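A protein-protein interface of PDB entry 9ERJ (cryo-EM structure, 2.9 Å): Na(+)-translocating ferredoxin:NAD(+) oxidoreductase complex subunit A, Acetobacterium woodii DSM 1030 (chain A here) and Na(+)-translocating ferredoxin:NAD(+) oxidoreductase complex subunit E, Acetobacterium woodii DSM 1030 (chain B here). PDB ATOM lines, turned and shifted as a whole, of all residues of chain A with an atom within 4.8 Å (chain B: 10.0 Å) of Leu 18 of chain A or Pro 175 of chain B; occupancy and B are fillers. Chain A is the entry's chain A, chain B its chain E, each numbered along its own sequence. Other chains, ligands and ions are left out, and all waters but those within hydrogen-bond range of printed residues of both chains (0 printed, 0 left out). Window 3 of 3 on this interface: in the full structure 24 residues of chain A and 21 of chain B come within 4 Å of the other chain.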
ATOM      1  N   ASN A  15      -2.935 -21.342  31.419  1.00  0.00           N
ATOM      2  CA  ASN A  15      -3.956 -22.383  31.343  1.00  0.00           C
ATOM      3  C   ASN A  15      -3.386 -23.667  30.751  1.00  0.00           C
ATOM      4  O   ASN A  15      -2.630 -23.634  29.777  1.00  0.00           O
ATOM      5  CB  ASN A  15      -5.130 -21.887  30.495  1.00  0.00           C
ATOM      6  CG  ASN A  15      -6.430 -22.590  30.826  1.00  0.00           C
ATOM      7  OD1 ASN A  15      -6.807 -23.558  30.169  1.00  0.00           O
ATOM      8  ND2 ASN A  15      -7.127 -22.097  31.840  1.00  0.00           N
ATOM      9  N   PHE A  16      -3.742 -24.800  31.360  1.00  0.00           N
ATOM     10  CA  PHE A  16      -3.120 -26.070  30.998  1.00  0.00           C
ATOM     11  C   PHE A  16      -3.540 -26.537  29.610  1.00  0.00           C
ATOM     12  O   PHE A  16      -2.724 -27.088  28.863  1.00  0.00           O
ATOM     13  CB  PHE A  16      -3.460 -27.134  32.042  1.00  0.00           C
ATOM     14  CG  PHE A  16      -2.367 -27.369  33.045  1.00  0.00           C
ATOM     15  CD1 PHE A  16      -1.736 -26.304  33.665  1.00  0.00           C
ATOM     16  CD2 PHE A  16      -1.971 -28.655  33.367  1.00  0.00           C
ATOM     17  CE1 PHE A  16      -0.731 -26.517  34.587  1.00  0.00           C
ATOM     18  CE2 PHE A  16      -0.965 -28.873  34.287  1.00  0.00           C
ATOM     19  CZ  PHE A  16      -0.345 -27.803  34.897  1.00  0.00           C
ATOM     20  N   VAL A  17      -4.806 -26.334  29.245  1.00  0.00           N
ATOM     21  CA  VAL A  17      -5.316 -26.890  27.994  1.00  0.00           C
ATOM     22  C   VAL A  17      -4.840 -26.066  26.804  1.00  0.00           C
ATOM     23  O   VAL A  17      -4.283 -26.599  25.838  1.00  0.00           O
ATOM     24  CB  VAL A  17      -6.851 -26.981  28.030  1.00  0.00           C
ATOM     25  CG1 VAL A  17      -7.348 -27.889  26.923  1.00  0.00           C
ATOM     26  CG2 VAL A  17      -7.319 -27.480  29.381  1.00  0.00           C
ATOM     27  N   LEU A  18      -5.060 -24.754  26.853  1.00  0.00           N
ATOM     28  CA  LEU A  18      -4.841 -23.921  25.674  1.00  0.00           C
ATOM     29  C   LEU A  18      -3.363 -23.603  25.474  1.00  0.00           C
ATOM     30  O   LEU A  18      -2.901 -23.459  24.336  1.00  0.00           O
ATOM     31  CB  LEU A  18      -5.674 -22.644  25.785  1.00  0.00           C
ATOM     32  CG  LEU A  18      -7.179 -22.901  25.915  1.00  0.00           C
ATOM     33  CD1 LEU A  18      -7.922 -21.642  26.303  1.00  0.00           C
ATOM     34  CD2 LEU A  18      -7.742 -23.476  24.625  1.00  0.00           C
ATOM     35  N   SER A  19      -2.603 -23.490  26.564  1.00  0.00           N
ATOM     36  CA  SER A  19      -1.209 -23.070  26.450  1.00  0.00           C
ATOM     37  C   SER A  19      -0.250 -24.257  26.460  1.00  0.00           C
ATOM     38  O   SER A  19       0.567 -24.415  25.547  1.00  0.00           O
ATOM     39  CB  SER A  19      -0.860 -22.093  27.575  1.00  0.00           C
ATOM     40  OG  SER A  19      -1.739 -20.983  27.577  1.00  0.00           O
ATOM     41  N   ARG A  20      -0.333 -25.102  27.485  1.00  0.00           N
ATOM     42  CA  ARG A  20       0.675 -26.129  27.715  1.00  0.00           C
ATOM     43  C   ARG A  20       0.396 -27.442  26.993  1.00  0.00           C
ATOM     44  O   ARG A  20       1.240 -28.342  27.054  1.00  0.00           O
ATOM     45  CB  ARG A  20       0.825 -26.391  29.216  1.00  0.00           C
ATOM     46  CG  ARG A  20       0.956 -25.130  30.050  1.00  0.00           C
ATOM     47  CD  ARG A  20       1.263 -25.455  31.500  1.00  0.00           C
ATOM     48  NE  ARG A  20       2.694 -25.608  31.733  1.00  0.00           N
ATOM     49  CZ  ARG A  20       3.359 -25.020  32.717  1.00  0.00           C
ATOM     50  NH1 ARG A  20       2.752 -24.231  33.588  1.00  0.00           N
ATOM     51  NH2 ARG A  20       4.667 -25.229  32.831  1.00  0.00           N
ATOM     52  N   PHE A  21      -0.756 -27.575  26.327  1.00  0.00           N
ATOM     53  CA  PHE A  21      -1.074 -28.728  25.479  1.00  0.00           C
ATOM     54  C   PHE A  21      -1.062 -30.036  26.273  1.00  0.00           C
ATOM     55  O   PHE A  21      -0.360 -30.988  25.932  1.00  0.00           O
ATOM     56  CB  PHE A  21      -0.105 -28.822  24.293  1.00  0.00           C
ATOM     57  CG  PHE A  21      -0.460 -27.943  23.136  1.00  0.00           C
ATOM     58  CD1 PHE A  21      -1.735 -27.948  22.606  1.00  0.00           C
ATOM     59  CD2 PHE A  21       0.496 -27.120  22.565  1.00  0.00           C
ATOM     60  CE1 PHE A  21      -2.052 -27.144  21.535  1.00  0.00           C
ATOM     61  CE2 PHE A  21       0.184 -26.313  21.494  1.00  0.00           C
ATOM     62  CZ  PHE A  21      -1.093 -26.324  20.979  1.00  0.00           C
ATOM     63  N   ALA A 176     -11.058 -24.537  18.940  1.00  0.00           N
ATOM     64  CA  ALA A 176      -9.995 -24.534  19.937  1.00  0.00           C
ATOM     65  C   ALA A 176      -8.885 -23.563  19.559  1.00  0.00           C
ATOM     66  O   ALA A 176      -8.319 -22.893  20.427  1.00  0.00           O
ATOM     67  CB  ALA A 176      -9.441 -25.945  20.119  1.00  0.00           C
ATOM     68  N   MET A 179     -10.167 -20.007  20.348  1.00  0.00           N
ATOM     69  CA  MET A 179     -10.075 -19.794  21.792  1.00  0.00           C
ATOM     70  C   MET A 179      -8.629 -19.641  22.249  1.00  0.00           C
ATOM     71  O   MET A 179      -8.348 -18.872  23.176  1.00  0.00           O
ATOM     72  CB  MET A 179     -10.744 -20.944  22.546  1.00  0.00           C
ATOM     73  CG  MET A 179     -12.209 -21.149  22.220  1.00  0.00           C
ATOM     74  SD  MET A 179     -12.901 -22.599  23.036  1.00  0.00           S
ATOM     75  CE  MET A 179     -12.576 -22.212  24.751  1.00  0.00           C
ATOM     76  N   ALA A 180      -7.702 -20.360  21.611  1.00  0.00           N
ATOM     77  CA  ALA A 180      -6.290 -20.222  21.941  1.00  0.00           C
ATOM     78  C   ALA A 180      -5.765 -18.834  21.604  1.00  0.00           C
ATOM     79  O   ALA A 180      -4.936 -18.300  22.339  1.00  0.00           O
ATOM     80  CB  ALA A 180      -5.474 -21.291  21.216  1.00  0.00           C
ATOM     81  N   PHE A 183      -7.110 -16.460  24.278  1.00  0.00           N
ATOM     82  CA  PHE A 183      -6.323 -16.579  25.501  1.00  0.00           C
ATOM     83  C   PHE A 183      -4.862 -16.178  25.313  1.00  0.00           C
ATOM     84  O   PHE A 183      -4.182 -15.899  26.306  1.00  0.00           O
ATOM     85  CB  PHE A 183      -6.407 -18.003  26.047  1.00  0.00           C
ATOM     86  CG  PHE A 183      -7.422 -18.167  27.140  1.00  0.00           C
ATOM     87  CD1 PHE A 183      -8.772 -18.223  26.846  1.00  0.00           C
ATOM     88  CD2 PHE A 183      -7.025 -18.255  28.463  1.00  0.00           C
ATOM     89  CE1 PHE A 183      -9.708 -18.372  27.849  1.00  0.00           C
ATOM     90  CE2 PHE A 183      -7.956 -18.402  29.471  1.00  0.00           C
ATOM     91  CZ  PHE A 183      -9.298 -18.461  29.164  1.00  0.00           C
ATOM     92  N   MET B  24      -2.834 -36.582  21.182  1.00  0.00           N
ATOM     93  CA  MET B  24      -2.867 -35.253  20.589  1.00  0.00           C
ATOM     94  C   MET B  24      -1.956 -34.250  21.281  1.00  0.00           C
ATOM     95  O   MET B  24      -1.767 -33.151  20.753  1.00  0.00           O
ATOM     96  CB  MET B  24      -4.301 -34.712  20.586  1.00  0.00           C
ATOM     97  CG  MET B  24      -5.171 -35.274  19.476  1.00  0.00           C
ATOM     98  SD  MET B  24      -4.767 -34.564  17.871  1.00  0.00           S
ATOM     99  CE  MET B  24      -4.823 -36.018  16.832  1.00  0.00           C
ATOM    100  N   CYS B  25      -1.394 -34.584  22.436  1.00  0.00           N
ATOM    101  CA  CYS B  25      -0.525 -33.627  23.110  1.00  0.00           C
ATOM    102  C   CYS B  25       0.863 -33.569  22.462  1.00  0.00           C
ATOM    103  O   CYS B  25       1.309 -32.465  22.116  1.00  0.00           O
ATOM    104  CB  CYS B  25      -0.438 -33.934  24.610  1.00  0.00           C
ATOM    105  SG  CYS B  25      -1.978 -34.534  25.339  1.00  0.00           S
ATOM    106  N   THR B  27       1.600 -34.517  19.449  1.00  0.00           N
ATOM    107  CA  THR B  27       1.383 -34.162  18.049  1.00  0.00           C
ATOM    108  C   THR B  27       1.300 -32.653  17.867  1.00  0.00           C
ATOM    109  O   THR B  27       1.904 -32.092  16.946  1.00  0.00           O
ATOM    110  CB  THR B  27       0.109 -34.833  17.534  1.00  0.00           C
ATOM    111  OG1 THR B  27       0.106 -36.214  17.910  1.00  0.00           O
ATOM    112  CG2 THR B  27       0.023 -34.724  16.022  1.00  0.00           C
ATOM    113  N   LEU B  28       0.552 -31.976  18.736  1.00  0.00           N
ATOM    114  CA  LEU B  28       0.450 -30.526  18.663  1.00  0.00           C
ATOM    115  C   LEU B  28       1.587 -29.818  19.385  1.00  0.00           C
ATOM    116  O   LEU B  28       1.750 -28.606  19.212  1.00  0.00           O
ATOM    117  CB  LEU B  28      -0.890 -30.064  19.238  1.00  0.00           C
ATOM    118  CG  LEU B  28      -2.140 -30.706  18.635  1.00  0.00           C
ATOM    119  CD1 LEU B  28      -3.369 -30.351  19.446  1.00  0.00           C
ATOM    120  CD2 LEU B  28      -2.315 -30.277  17.192  1.00  0.00           C
ATOM    121  N   ALA B  29       2.380 -30.536  20.181  1.00  0.00           N
ATOM    122  CA  ALA B  29       3.412 -29.885  20.976  1.00  0.00           C
ATOM    123  C   ALA B  29       4.783 -29.883  20.309  1.00  0.00           C
ATOM    124  O   ALA B  29       5.487 -28.869  20.359  1.00  0.00           O
ATOM    125  CB  ALA B  29       3.510 -30.552  22.349  1.00  0.00           C
ATOM    126  N   VAL B  30       5.189 -30.992  19.683  1.00  0.00           N
ATOM    127  CA  VAL B  30       6.569 -31.129  19.220  1.00  0.00           C
ATOM    128  C   VAL B  30       6.728 -30.958  17.715  1.00  0.00           C
ATOM    129  O   VAL B  30       7.870 -30.895  17.233  1.00  0.00           O
ATOM    130  CB  VAL B  30       7.167 -32.488  19.647  1.00  0.00           C
ATOM    131  CG1 VAL B  30       6.820 -32.787  21.096  1.00  0.00           C
ATOM    132  CG2 VAL B  30       6.693 -33.601  18.727  1.00  0.00           C
ATOM    133  N   THR B  31       5.634 -30.870  16.958  1.00  0.00           N
ATOM    134  CA  THR B  31       5.710 -30.830  15.497  1.00  0.00           C
ATOM    135  C   THR B  31       5.939 -29.404  14.989  1.00  0.00           C
ATOM    136  O   THR B  31       5.160 -28.849  14.216  1.00  0.00           O
ATOM    137  CB  THR B  31       4.452 -31.430  14.886  1.00  0.00           C
ATOM    138  OG1 THR B  31       3.298 -30.907  15.554  1.00  0.00           O
ATOM    139  CG2 THR B  31       4.466 -32.942  15.021  1.00  0.00           C
ATOM    140  N   THR B  32       7.041 -28.809  15.442  1.00  0.00           N
ATOM    141  CA  THR B  32       7.511 -27.536  14.914  1.00  0.00           C
ATOM    142  C   THR B  32       8.672 -27.705  13.946  1.00  0.00           C
ATOM    143  O   THR B  32       9.201 -26.706  13.451  1.00  0.00           O
ATOM    144  CB  THR B  32       7.925 -26.599  16.054  1.00  0.00           C
ATOM    145  OG1 THR B  32       9.220 -26.975  16.539  1.00  0.00           O
ATOM    146  CG2 THR B  32       6.924 -26.666  17.194  1.00  0.00           C
ATOM    147  N   ARG B 148       4.119 -27.524   8.840  1.00  0.00           N
ATOM    148  CA  ARG B 148       4.257 -26.371   9.726  1.00  0.00           C
ATOM    149  C   ARG B 148       5.593 -25.662   9.527  1.00  0.00           C
ATOM    150  O   ARG B 148       5.649 -24.426   9.538  1.00  0.00           O
ATOM    151  CB  ARG B 148       4.088 -26.797  11.183  1.00  0.00           C
ATOM    152  CG  ARG B 148       2.666 -26.668  11.698  1.00  0.00           C
ATOM    153  CD  ARG B 148       2.526 -27.242  13.094  1.00  0.00           C
ATOM    154  NE  ARG B 148       2.878 -26.272  14.124  1.00  0.00           N
ATOM    155  CZ  ARG B 148       2.940 -26.546  15.420  1.00  0.00           C
ATOM    156  NH1 ARG B 148       2.682 -27.758  15.882  1.00  0.00           N
ATOM    157  NH2 ARG B 148       3.269 -25.581  16.273  1.00  0.00           N
ATOM    158  N   LEU B 170       4.969 -16.230  11.876  1.00  0.00           N
ATOM    159  CA  LEU B 170       5.387 -16.690  13.193  1.00  0.00           C
ATOM    160  C   LEU B 170       4.228 -17.172  14.058  1.00  0.00           C
ATOM    161  O   LEU B 170       4.407 -17.354  15.267  1.00  0.00           O
ATOM    162  CB  LEU B 170       6.155 -15.583  13.921  1.00  0.00           C
ATOM    163  CG  LEU B 170       7.470 -15.138  13.283  1.00  0.00           C
ATOM    164  CD1 LEU B 170       7.973 -13.863  13.934  1.00  0.00           C
ATOM    165  CD2 LEU B 170       8.510 -16.238  13.378  1.00  0.00           C
ATOM    166  N   LEU B 171       3.047 -17.378  13.476  1.00  0.00           N
ATOM    167  CA  LEU B 171       1.943 -17.988  14.202  1.00  0.00           C
ATOM    168  C   LEU B 171       1.896 -19.501  14.044  1.00  0.00           C
ATOM    169  O   LEU B 171       1.348 -20.182  14.916  1.00  0.00           O
ATOM    170  CB  LEU B 171       0.604 -17.395  13.745  1.00  0.00           C
ATOM    171  CG  LEU B 171      -0.599 -17.621  14.666  1.00  0.00           C
ATOM    172  CD1 LEU B 171      -0.684 -16.539  15.727  1.00  0.00           C
ATOM    173  CD2 LEU B 171      -1.891 -17.700  13.870  1.00  0.00           C
ATOM    174  N   MET B 172       2.476 -20.041  12.970  1.00  0.00           N
ATOM    175  CA  MET B 172       2.486 -21.482  12.754  1.00  0.00           C
ATOM    176  C   MET B 172       3.380 -22.220  13.738  1.00  0.00           C
ATOM    177  O   MET B 172       3.205 -23.428  13.928  1.00  0.00           O
ATOM    178  CB  MET B 172       2.929 -21.792  11.324  1.00  0.00           C
ATOM    179  CG  MET B 172       2.202 -20.983  10.271  1.00  0.00           C
ATOM    180  SD  MET B 172       0.635 -21.735   9.812  1.00  0.00           S
ATOM    181  CE  MET B 172       1.210 -23.291   9.140  1.00  0.00           C
ATOM    182  N   ILE B 173       4.326 -21.529  14.364  1.00  0.00           N
ATOM    183  CA  ILE B 173       5.168 -22.118  15.394  1.00  0.00           C
ATOM    184  C   ILE B 173       4.676 -21.744  16.793  1.00  0.00           C
ATOM    185  O   ILE B 173       5.440 -21.801  17.756  1.00  0.00           O
ATOM    186  CB  ILE B 173       6.642 -21.736  15.198  1.00  0.00           C
ATOM    187  CG1 ILE B 173       6.804 -20.215  15.221  1.00  0.00           C
ATOM    188  CG2 ILE B 173       7.171 -22.314  13.897  1.00  0.00           C
ATOM    189  CD1 ILE B 173       8.228 -19.752  15.046  1.00  0.00           C
ATOM    190  N   LEU B 174       3.411 -21.367  16.916  1.00  0.00           N
ATOM    191  CA  LEU B 174       2.768 -20.985  18.161  1.00  0.00           C
ATOM    192  C   LEU B 174       1.656 -21.979  18.475  1.00  0.00           C
ATOM    193  O   LEU B 174       1.225 -22.732  17.593  1.00  0.00           O
ATOM    194  CB  LEU B 174       2.199 -19.561  18.058  1.00  0.00           C
ATOM    195  CG  LEU B 174       3.201 -18.410  18.194  1.00  0.00           C
ATOM    196  CD1 LEU B 174       2.481 -17.099  18.468  1.00  0.00           C
ATOM    197  CD2 LEU B 174       4.229 -18.696  19.278  1.00  0.00           C
ATOM    198  N   PRO B 175       1.198 -22.041  19.726  1.00  0.00           N
ATOM    199  CA  PRO B 175       0.118 -22.981  20.091  1.00  0.00           C
ATOM    200  C   PRO B 175      -1.148 -22.823  19.257  1.00  0.00           C
ATOM    201  O   PRO B 175      -1.756 -23.844  18.900  1.00  0.00           O
ATOM    202  CB  PRO B 175      -0.136 -22.663  21.573  1.00  0.00           C
ATOM    203  CG  PRO B 175       1.185 -22.220  22.070  1.00  0.00           C
ATOM    204  CD  PRO B 175       1.852 -21.486  20.929  1.00  0.00           C
ATOM    205  N   PRO B 176      -1.606 -21.610  18.914  1.00  0.00           N
ATOM    206  CA  PRO B 176      -2.800 -21.529  18.057  1.00  0.00           C
ATOM    207  C   PRO B 176      -2.567 -21.903  16.603  1.00  0.00           C
ATOM    208  O   PRO B 176      -3.545 -22.104  15.875  1.00  0.00           O
ATOM    209  CB  PRO B 176      -3.218 -20.053  18.175  1.00  0.00           C
ATOM    210  CG  PRO B 176      -2.547 -19.556  19.377  1.00  0.00           C
ATOM    211  CD  PRO B 176      -1.247 -20.255  19.380  1.00  0.00           C
ATOM    212  N   GLY B 177      -1.321 -22.007  16.153  1.00  0.00           N
ATOM    213  CA  GLY B 177      -1.053 -22.306  14.760  1.00  0.00           C
ATOM    214  C   GLY B 177      -1.088 -23.784  14.440  1.00  0.00           C
ATOM    215  O   GLY B 177      -1.063 -24.174  13.270  1.00  0.00           O
ATOM    216  N   ALA B 178      -1.140 -24.620  15.475  1.00  0.00           N
ATOM    217  CA  ALA B 178      -1.235 -26.060  15.283  1.00  0.00           C
ATOM    218  C   ALA B 178      -2.663 -26.508  15.005  1.00  0.00           C
ATOM    219  O   ALA B 178      -2.933 -27.040  13.918  1.00  0.00           O
ATOM    220  CB  ALA B 178      -0.690 -26.793  16.510  1.00  0.00           C
ATOM    221  N   PHE B 179      -3.565 -26.246  15.968  1.00  0.00           N
ATOM    222  CA  PHE B 179      -4.957 -26.697  15.912  1.00  0.00           C
ATOM    223  C   PHE B 179      -5.550 -26.524  14.524  1.00  0.00           C
ATOM    224  O   PHE B 179      -5.864 -27.513  13.844  1.00  0.00           O
ATOM    225  CB  PHE B 179      -5.803 -25.908  16.914  1.00  0.00           C
ATOM    226  CG  PHE B 179      -5.690 -26.375  18.333  1.00  0.00           C
ATOM    227  CD1 PHE B 179      -6.139 -27.629  18.706  1.00  0.00           C
ATOM    228  CD2 PHE B 179      -5.180 -25.536  19.307  1.00  0.00           C
ATOM    229  CE1 PHE B 179      -6.055 -28.047  20.019  1.00  0.00           C
ATOM    230  CE2 PHE B 179      -5.095 -25.946  20.621  1.00  0.00           C
ATOM    231  CZ  PHE B 179      -5.531 -27.203  20.976  1.00  0.00           C
ATOM    232  N   LEU B 180      -5.623 -25.269  14.064  1.00  0.00           N
ATOM    233  CA  LEU B 180      -6.260 -24.941  12.793  1.00  0.00           C
ATOM    234  C   LEU B 180      -5.717 -25.810  11.672  1.00  0.00           C
ATOM    235  O   LEU B 180      -6.486 -26.499  10.984  1.00  0.00           O
ATOM    236  CB  LEU B 180      -6.042 -23.461  12.468  1.00  0.00           C
ATOM    237  CG  LEU B 180      -6.392 -22.409  13.525  1.00  0.00           C
ATOM    238  CD1 LEU B 180      -5.821 -21.058  13.133  1.00  0.00           C
ATOM    239  CD2 LEU B 180      -7.891 -22.307  13.729  1.00  0.00           C
ATOM    240  N   THR B 181      -4.384 -25.874  11.550  1.00  0.00           N
ATOM    241  CA  THR B 181      -3.776 -26.632  10.462  1.00  0.00           C
ATOM    242  C   THR B 181      -4.230 -28.080  10.495  1.00  0.00           C
ATOM    243  O   THR B 181      -4.764 -28.586   9.497  1.00  0.00           O
ATOM    244  CB  THR B 181      -2.253 -26.551  10.540  1.00  0.00           C
ATOM    245  OG1 THR B 181      -1.824 -26.849  11.872  1.00  0.00           O
ATOM    246  CG2 THR B 181      -1.779 -25.163  10.164  1.00  0.00           C
ATOM    247  N   LEU B 182      -4.136 -28.716  11.671  1.00  0.00           N
ATOM    248  CA  LEU B 182      -4.529 -30.114  11.779  1.00  0.00           C
ATOM    249  C   LEU B 182      -5.979 -30.291  11.371  1.00  0.00           C
ATOM    250  O   LEU B 182      -6.293 -31.173  10.558  1.00  0.00           O
ATOM    251  CB  LEU B 182      -4.300 -30.624  13.200  1.00  0.00           C
ATOM    252  CG  LEU B 182      -4.473 -32.131  13.403  1.00  0.00           C
ATOM    253  CD1 LEU B 182      -3.608 -32.913  12.431  1.00  0.00           C
ATOM    254  CD2 LEU B 182      -4.155 -32.520  14.836  1.00  0.00           C
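The backbone carbonyl oxygen (O) of Phe 16 of chain A sits at hydrogen-bond distance from the backbone NH (N) of Phe 21 of chain A (3.2 Å).
Printed residues of chain B that touch a printed residue of chain A: Cys 25, Leu 28, Pro 175, Pro 176 and Phe 179.
Hydrophobic or aromatic side chains of chain B within 4 Å of the printed part of chain A: Leu 28, Pro 175, Pro 176 and Phe 179.
Along chain B the printed residues that touch a printed residue of chain A span positions 25 to 179.
Among the printed residues, no Asp or Glu carboxylate lies within 4 Å of a Lys or Arg side-chain nitrogen of the other chain.
Pro 175 of chain B touches Leu 18 of chain A (CB to O, 3.99 Å).
Cys 25 of chain B touches Phe 21 of chain A.
Phe 21 of chain A touches Leu 28 of chain B.
Phe 21 of chain A touches Pro 175 of chain B.
Phe 179 of chain B touches Phe 21 of chain A.
CB of Ala 176 of chain A touches CD1 of Phe 179 of chain B (3.97 Å).
Ala 180 of chain A touches Pro 176 of chain B.
Val 17 of chain A touches none of the printed residues of chain B.
Of the printed residues of chain B, Leu 18 of chain A touches Pro 175.
No residue of chain B comes within 4 Å of Ser 19 of chain A.
Printed residues of chain B within 4 Å of Phe 21 of chain A: Cys 25, Leu 28, Pro 175 and Phe 179.
Printed residues of chain B within 4 Å of Ala 176 of chain A: Phe 179 (3.97 Å).
Ala 180 of chain A touches one residue of chain B.
Of the printed residues of chain A, Leu 28 of chain B touches Phe 21 (3.6 Å).
Printed residues of chain A within 4 Å of Pro 175 of chain B: Leu 18 and Phe 21.
Printed residues of chain A within 4 Å of Pro 176 of chain B: Ala 180.
Of the printed residues of chain A, Phe 179 of chain B touches Phe 21 (3.4 Å) and Ala 176 (3.97 Å).
The nearest printed residue of chain A that does not touch Pro 175 of chain B is Ser 19 of chain A (4.2 Å).
The nearest printed residue of chain A that does not touch Phe 179 of chain B is Ala 180 of chain A (4.7 Å).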
